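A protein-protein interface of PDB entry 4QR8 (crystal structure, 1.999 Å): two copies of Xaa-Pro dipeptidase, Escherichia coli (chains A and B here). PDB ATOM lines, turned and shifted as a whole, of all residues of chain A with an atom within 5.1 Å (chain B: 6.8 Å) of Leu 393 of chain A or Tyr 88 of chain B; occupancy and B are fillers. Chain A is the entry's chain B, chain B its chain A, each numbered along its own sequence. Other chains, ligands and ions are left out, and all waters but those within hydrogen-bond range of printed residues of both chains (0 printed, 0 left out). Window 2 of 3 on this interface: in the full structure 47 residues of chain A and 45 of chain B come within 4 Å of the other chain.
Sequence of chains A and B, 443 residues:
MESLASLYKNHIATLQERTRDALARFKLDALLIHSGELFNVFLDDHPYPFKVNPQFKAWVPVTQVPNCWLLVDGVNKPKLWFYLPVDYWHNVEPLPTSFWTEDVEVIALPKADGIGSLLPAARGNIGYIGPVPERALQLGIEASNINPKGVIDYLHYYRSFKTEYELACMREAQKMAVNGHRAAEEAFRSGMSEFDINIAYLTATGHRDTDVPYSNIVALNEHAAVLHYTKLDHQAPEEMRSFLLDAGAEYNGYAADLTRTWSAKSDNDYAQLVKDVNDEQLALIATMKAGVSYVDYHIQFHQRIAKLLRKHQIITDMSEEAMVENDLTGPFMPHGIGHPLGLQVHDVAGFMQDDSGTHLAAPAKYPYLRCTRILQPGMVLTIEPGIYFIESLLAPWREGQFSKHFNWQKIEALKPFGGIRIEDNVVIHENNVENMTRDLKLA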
ATOM      1  N   ALA A 225      -7.471 -22.863   8.907  1.00  0.00           N
ATOM      2  CA  ALA A 225      -7.347 -22.255  10.231  1.00  0.00           C
ATOM      3  C   ALA A 225      -8.709 -21.854  10.798  1.00  0.00           C
ATOM      4  O   ALA A 225      -8.819 -21.493  11.970  1.00  0.00           O
ATOM      5  CB  ALA A 225      -6.416 -21.047  10.180  1.00  0.00           C
ATOM      6  N   VAL A 226      -9.740 -21.917   9.962  1.00  0.00           N
ATOM      7  CA  VAL A 226     -11.093 -21.564  10.387  1.00  0.00           C
ATOM      8  C   VAL A 226     -11.848 -22.814  10.821  1.00  0.00           C
ATOM      9  O   VAL A 226     -12.206 -23.651   9.987  1.00  0.00           O
ATOM     10  CB  VAL A 226     -11.873 -20.868   9.256  1.00  0.00           C
ATOM     11  CG1 VAL A 226     -13.266 -20.469   9.731  1.00  0.00           C
ATOM     12  CG2 VAL A 226     -11.105 -19.656   8.751  1.00  0.00           C
ATOM     13  N   LEU A 227     -12.094 -22.931  12.125  1.00  0.00           N
ATOM     14  CA  LEU A 227     -12.659 -24.150  12.700  1.00  0.00           C
ATOM     15  C   LEU A 227     -14.023 -24.536  12.128  1.00  0.00           C
ATOM     16  O   LEU A 227     -14.240 -25.692  11.767  1.00  0.00           O
ATOM     17  CB  LEU A 227     -12.715 -24.061  14.228  1.00  0.00           C
ATOM     18  CG  LEU A 227     -11.342 -24.019  14.909  1.00  0.00           C
ATOM     19  CD1 LEU A 227     -11.477 -24.175  16.416  1.00  0.00           C
ATOM     20  CD2 LEU A 227     -10.428 -25.094  14.330  1.00  0.00           C
ATOM     21  N   PRO A 331      -3.385 -21.603  22.373  1.00  0.00           N
ATOM     22  CA  PRO A 331      -3.851 -21.011  21.113  1.00  0.00           C
ATOM     23  C   PRO A 331      -3.639 -21.907  19.895  1.00  0.00           C
ATOM     24  O   PRO A 331      -4.229 -21.648  18.845  1.00  0.00           O
ATOM     25  CB  PRO A 331      -2.989 -19.751  20.984  1.00  0.00           C
ATOM     26  CG  PRO A 331      -1.761 -20.063  21.754  1.00  0.00           C
ATOM     27  CD  PRO A 331      -2.242 -20.859  22.930  1.00  0.00           C
ATOM     28  N   PRO A 334      -7.328 -24.512  20.121  1.00  0.00           N
ATOM     29  CA  PRO A 334      -8.372 -23.850  20.907  1.00  0.00           C
ATOM     30  C   PRO A 334      -9.697 -24.601  20.851  1.00  0.00           C
ATOM     31  O   PRO A 334     -10.755 -23.975  20.785  1.00  0.00           O
ATOM     32  CB  PRO A 334      -8.506 -22.492  20.218  1.00  0.00           C
ATOM     33  CG  PRO A 334      -8.191 -22.788  18.785  1.00  0.00           C
ATOM     34  CD  PRO A 334      -7.152 -23.882  18.798  1.00  0.00           C
ATOM     35  N   TYR A 368     -13.484 -25.279  26.148  1.00  0.00           N
ATOM     36  CA  TYR A 368     -14.202 -25.786  24.982  1.00  0.00           C
ATOM     37  C   TYR A 368     -14.141 -27.307  24.834  1.00  0.00           C
ATOM     38  O   TYR A 368     -14.575 -27.856  23.816  1.00  0.00           O
ATOM     39  CB  TYR A 368     -13.734 -25.072  23.708  1.00  0.00           C
ATOM     40  CG  TYR A 368     -13.924 -23.573  23.792  1.00  0.00           C
ATOM     41  CD1 TYR A 368     -15.197 -23.018  23.817  1.00  0.00           C
ATOM     42  CD2 TYR A 368     -12.833 -22.717  23.874  1.00  0.00           C
ATOM     43  CE1 TYR A 368     -15.382 -21.651  23.908  1.00  0.00           C
ATOM     44  CE2 TYR A 368     -13.007 -21.345  23.963  1.00  0.00           C
ATOM     45  CZ  TYR A 368     -14.284 -20.819  23.980  1.00  0.00           C
ATOM     46  OH  TYR A 368     -14.469 -19.457  24.069  1.00  0.00           O
ATOM     47  N   ILE A 390      -3.607 -19.363  14.102  1.00  0.00           N
ATOM     48  CA  ILE A 390      -4.681 -18.381  14.066  1.00  0.00           C
ATOM     49  C   ILE A 390      -4.218 -17.065  14.675  1.00  0.00           C
ATOM     50  O   ILE A 390      -3.994 -16.977  15.883  1.00  0.00           O
ATOM     51  CB  ILE A 390      -5.897 -18.889  14.855  1.00  0.00           C
ATOM     52  CG1 ILE A 390      -6.250 -20.315  14.417  1.00  0.00           C
ATOM     53  CG2 ILE A 390      -7.077 -17.944  14.684  1.00  0.00           C
ATOM     54  CD1 ILE A 390      -7.207 -21.029  15.354  1.00  0.00           C
ATOM     55  N   GLU A 391      -4.081 -16.045  13.831  1.00  0.00           N
ATOM     56  CA  GLU A 391      -3.519 -14.762  14.247  1.00  0.00           C
ATOM     57  C   GLU A 391      -4.252 -14.110  15.421  1.00  0.00           C
ATOM     58  O   GLU A 391      -3.615 -13.564  16.318  1.00  0.00           O
ATOM     59  CB  GLU A 391      -3.443 -13.789  13.065  1.00  0.00           C
ATOM     60  CG  GLU A 391      -2.813 -12.436  13.407  1.00  0.00           C
ATOM     61  CD  GLU A 391      -1.311 -12.521  13.664  1.00  0.00           C
ATOM     62  OE1 GLU A 391      -0.711 -13.588  13.404  1.00  0.00           O
ATOM     63  OE2 GLU A 391      -0.726 -11.513  14.120  1.00  0.00           O
ATOM     64  N   SER A 392      -5.580 -14.179  15.425  1.00  0.00           N
ATOM     65  CA  SER A 392      -6.358 -13.536  16.480  1.00  0.00           C
ATOM     66  C   SER A 392      -6.049 -14.116  17.860  1.00  0.00           C
ATOM     67  O   SER A 392      -6.155 -13.418  18.867  1.00  0.00           O
ATOM     68  CB  SER A 392      -7.864 -13.594  16.185  1.00  0.00           C
ATOM     69  OG  SER A 392      -8.390 -14.899  16.362  1.00  0.00           O
ATOM     70  N   LEU A 393      -5.645 -15.383  17.901  1.00  0.00           N
ATOM     71  CA  LEU A 393      -5.295 -16.025  19.168  1.00  0.00           C
ATOM     72  C   LEU A 393      -3.812 -15.893  19.509  1.00  0.00           C
ATOM     73  O   LEU A 393      -3.443 -15.829  20.681  1.00  0.00           O
ATOM     74  CB  LEU A 393      -5.701 -17.500  19.157  1.00  0.00           C
ATOM     75  CG  LEU A 393      -7.205 -17.764  19.082  1.00  0.00           C
ATOM     76  CD1 LEU A 393      -7.477 -19.249  18.965  1.00  0.00           C
ATOM     77  CD2 LEU A 393      -7.908 -17.190  20.299  1.00  0.00           C
ATOM     78  N   LEU A 394      -2.963 -15.849  18.486  1.00  0.00           N
ATOM     79  CA  LEU A 394      -1.516 -15.801  18.692  1.00  0.00           C
ATOM     80  C   LEU A 394      -0.997 -14.396  19.010  1.00  0.00           C
ATOM     81  O   LEU A 394      -0.124 -14.228  19.860  1.00  0.00           O
ATOM     82  CB  LEU A 394      -0.782 -16.374  17.473  1.00  0.00           C
ATOM     83  CG  LEU A 394      -0.895 -17.887  17.282  1.00  0.00           C
ATOM     84  CD1 LEU A 394      -0.267 -18.323  15.961  1.00  0.00           C
ATOM     85  CD2 LEU A 394      -0.254 -18.628  18.450  1.00  0.00           C
ATOM     86  N   ALA A 395      -1.538 -13.396  18.322  1.00  0.00           N
ATOM     87  CA  ALA A 395      -1.098 -12.007  18.487  1.00  0.00           C
ATOM     88  C   ALA A 395      -1.051 -11.459  19.927  1.00  0.00           C
ATOM     89  O   ALA A 395      -0.082 -10.793  20.289  1.00  0.00           O
ATOM     90  CB  ALA A 395      -1.905 -11.072  17.574  1.00  0.00           C
ATOM     91  N   PRO A 396      -2.088 -11.725  20.749  1.00  0.00           N
ATOM     92  CA  PRO A 396      -2.028 -11.196  22.119  1.00  0.00           C
ATOM     93  C   PRO A 396      -0.800 -11.642  22.913  1.00  0.00           C
ATOM     94  O   PRO A 396      -0.377 -10.923  23.818  1.00  0.00           O
ATOM     95  CB  PRO A 396      -3.300 -11.750  22.761  1.00  0.00           C
ATOM     96  CG  PRO A 396      -4.249 -11.890  21.621  1.00  0.00           C
ATOM     97  CD  PRO A 396      -3.402 -12.333  20.462  1.00  0.00           C
ATOM     98  N   TRP A 397      -0.231 -12.795  22.576  1.00  0.00           N
ATOM     99  CA  TRP A 397       0.952 -13.284  23.272  1.00  0.00           C
ATOM    100  C   TRP A 397       2.169 -12.383  23.065  1.00  0.00           C
ATOM    101  O   TRP A 397       3.117 -12.432  23.849  1.00  0.00           O
ATOM    102  CB  TRP A 397       1.272 -14.723  22.861  1.00  0.00           C
ATOM    103  CG  TRP A 397       0.261 -15.712  23.358  1.00  0.00           C
ATOM    104  CD1 TRP A 397      -0.939 -16.013  22.787  1.00  0.00           C
ATOM    105  CD2 TRP A 397       0.362 -16.523  24.535  1.00  0.00           C
ATOM    106  NE1 TRP A 397      -1.593 -16.965  23.534  1.00  0.00           N
ATOM    107  CE2 TRP A 397      -0.812 -17.297  24.613  1.00  0.00           C
ATOM    108  CE3 TRP A 397       1.334 -16.672  25.531  1.00  0.00           C
ATOM    109  CZ2 TRP A 397      -1.044 -18.204  25.645  1.00  0.00           C
ATOM    110  CZ3 TRP A 397       1.105 -17.575  26.554  1.00  0.00           C
ATOM    111  CH2 TRP A 397      -0.074 -18.329  26.603  1.00  0.00           C
ATOM    112  N   VAL B  86     -16.552 -11.003  15.444  1.00  0.00           N
ATOM    113  CA  VAL B  86     -15.132 -11.302  15.366  1.00  0.00           C
ATOM    114  C   VAL B  86     -14.853 -12.553  16.188  1.00  0.00           C
ATOM    115  O   VAL B  86     -14.689 -12.485  17.403  1.00  0.00           O
ATOM    116  CB  VAL B  86     -14.276 -10.123  15.865  1.00  0.00           C
ATOM    117  CG1 VAL B  86     -12.796 -10.470  15.806  1.00  0.00           C
ATOM    118  CG2 VAL B  86     -14.567  -8.876  15.039  1.00  0.00           C
ATOM    119  N   ASP B  87     -14.832 -13.701  15.519  1.00  0.00           N
ATOM    120  CA  ASP B  87     -14.564 -14.970  16.188  1.00  0.00           C
ATOM    121  C   ASP B  87     -13.814 -15.934  15.271  1.00  0.00           C
ATOM    122  O   ASP B  87     -14.067 -15.989  14.068  1.00  0.00           O
ATOM    123  CB  ASP B  87     -15.859 -15.602  16.708  1.00  0.00           C
ATOM    124  CG  ASP B  87     -16.736 -16.145  15.598  1.00  0.00           C
ATOM    125  OD1 ASP B  87     -16.854 -15.486  14.541  1.00  0.00           O
ATOM    126  OD2 ASP B  87     -17.310 -17.238  15.786  1.00  0.00           O
ATOM    127  N   TYR B  88     -12.894 -16.696  15.851  1.00  0.00           N
ATOM    128  CA  TYR B  88     -12.001 -17.546  15.074  1.00  0.00           C
ATOM    129  C   TYR B  88     -12.659 -18.858  14.653  1.00  0.00           C
ATOM    130  O   TYR B  88     -12.062 -19.645  13.912  1.00  0.00           O
ATOM    131  CB  TYR B  88     -10.720 -17.830  15.864  1.00  0.00           C
ATOM    132  CG  TYR B  88     -10.933 -18.606  17.148  1.00  0.00           C
ATOM    133  CD1 TYR B  88     -10.849 -19.994  17.167  1.00  0.00           C
ATOM    134  CD2 TYR B  88     -11.209 -17.952  18.342  1.00  0.00           C
ATOM    135  CE1 TYR B  88     -11.040 -20.708  18.336  1.00  0.00           C
ATOM    136  CE2 TYR B  88     -11.399 -18.658  19.518  1.00  0.00           C
ATOM    137  CZ  TYR B  88     -11.314 -20.035  19.507  1.00  0.00           C
ATOM    138  OH  TYR B  88     -11.501 -20.741  20.670  1.00  0.00           O
ATOM    139  N   TRP B  89     -13.882 -19.091  15.125  1.00  0.00           N
ATOM    140  CA  TRP B  89     -14.588 -20.338  14.835  1.00  0.00           C
ATOM    141  C   TRP B  89     -15.144 -20.359  13.422  1.00  0.00           C
ATOM    142  O   TRP B  89     -14.796 -21.219  12.619  1.00  0.00           O
ATOM    143  CB  TRP B  89     -15.753 -20.548  15.806  1.00  0.00           C
ATOM    144  CG  TRP B  89     -15.426 -20.271  17.234  1.00  0.00           C
ATOM    145  CD1 TRP B  89     -15.422 -19.060  17.849  1.00  0.00           C
ATOM    146  CD2 TRP B  89     -15.058 -21.240  18.234  1.00  0.00           C
ATOM    147  NE1 TRP B  89     -15.063 -19.212  19.182  1.00  0.00           N
ATOM    148  CE2 TRP B  89     -14.836 -20.539  19.437  1.00  0.00           C
ATOM    149  CE3 TRP B  89     -14.889 -22.634  18.223  1.00  0.00           C
ATOM    150  CZ2 TRP B  89     -14.462 -21.177  20.613  1.00  0.00           C
ATOM    151  CZ3 TRP B  89     -14.512 -23.267  19.395  1.00  0.00           C
ATOM    152  CH2 TRP B  89     -14.302 -22.534  20.575  1.00  0.00           C
ATOM    153  N   HIS B  90     -16.024 -19.408  13.129  1.00  0.00           N
ATOM    154  CA  HIS B  90     -16.788 -19.433  11.887  1.00  0.00           C
ATOM    155  C   HIS B  90     -16.201 -18.546  10.795  1.00  0.00           C
ATOM    156  O   HIS B  90     -15.443 -17.614  11.074  1.00  0.00           O
ATOM    157  CB  HIS B  90     -18.241 -19.019  12.147  1.00  0.00           C
ATOM    158  CG  HIS B  90     -18.879 -19.734  13.296  1.00  0.00           C
ATOM    159  ND1 HIS B  90     -19.487 -20.963  13.161  1.00  0.00           N
ATOM    160  CD2 HIS B  90     -19.012 -19.392  14.600  1.00  0.00           C
ATOM    161  CE1 HIS B  90     -19.962 -21.350  14.331  1.00  0.00           C
ATOM    162  NE2 HIS B  90     -19.687 -20.413  15.221  1.00  0.00           N
ATOM    163  N   ASN B  91     -16.556 -18.855   9.551  1.00  0.00           N
ATOM    164  CA  ASN B  91     -16.286 -17.963   8.434  1.00  0.00           C
ATOM    165  C   ASN B  91     -17.268 -16.802   8.497  1.00  0.00           C
ATOM    166  O   ASN B  91     -18.466 -17.002   8.706  1.00  0.00           O
ATOM    167  CB  ASN B  91     -16.392 -18.706   7.098  1.00  0.00           C
ATOM    168  CG  ASN B  91     -17.700 -19.461   6.952  1.00  0.00           C
ATOM    169  OD1 ASN B  91     -17.812 -20.621   7.354  1.00  0.00           O
ATOM    170  ND2 ASN B  91     -18.700 -18.805   6.372  1.00  0.00           N
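OH of Tyr 88 of chain B sits at hydrogen-bond distance from O of Pro 334 of chain A, at 3.3 Å. The backbone NH (N) of Leu 227 of chain A is in hydrogen-bond range of the backbone carbonyl oxygen (O) of Trp 89 of chain B.
Among the printed residues, pairs that only touch across the chains: Val 226 of chain A with Trp 89 of chain B (3.4 Å), Val 226 of chain A with His 90 of chain B (3.7 Å), Val 226 of chain A with Asn 91 of chain B (3.7 Å), Leu 227 of chain A with Tyr 88 of chain B (3.7 Å), Pro 334 of chain A with Trp 89 of chain B (3.8 Å), Tyr 368 of chain A with Tyr 88 of chain B (3.7 Å), Tyr 368 of chain A with Trp 89 of chain B (3.4 Å), Ile 390 of chain A with Tyr 88 of chain B (3.8 Å), Ser 392 of chain A with Tyr 88 of chain B (3.8 Å) and Leu 393 of chain A with Tyr 88 of chain B (3.9 Å).
Tyr 88 of chain B touches just these residues of chain A: Leu 227, Pro 334, Tyr 368, Ile 390, Ser 392 and Leu 393. Of the printed residues of chain B, Ile 390 of chain A touches Tyr 88. Of the printed residues of chain A, His 90 of chain B touches Val 226 (3.7 Å). Trp 397 of chain A touches none of the printed residues of chain B. Ala 225 of chain A touches none of the printed residues of chain B. The nearest printed residue of chain B that does not touch Leu 393 of chain A is Trp 89 of chain B (7.4 Å).
Printed residues of chain B that touch a printed residue of chain A: Tyr 88, Trp 89, His 90 and Asn 91. Among the printed residues, 12 pairs touch across the chains.
No position is printed for both chains.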
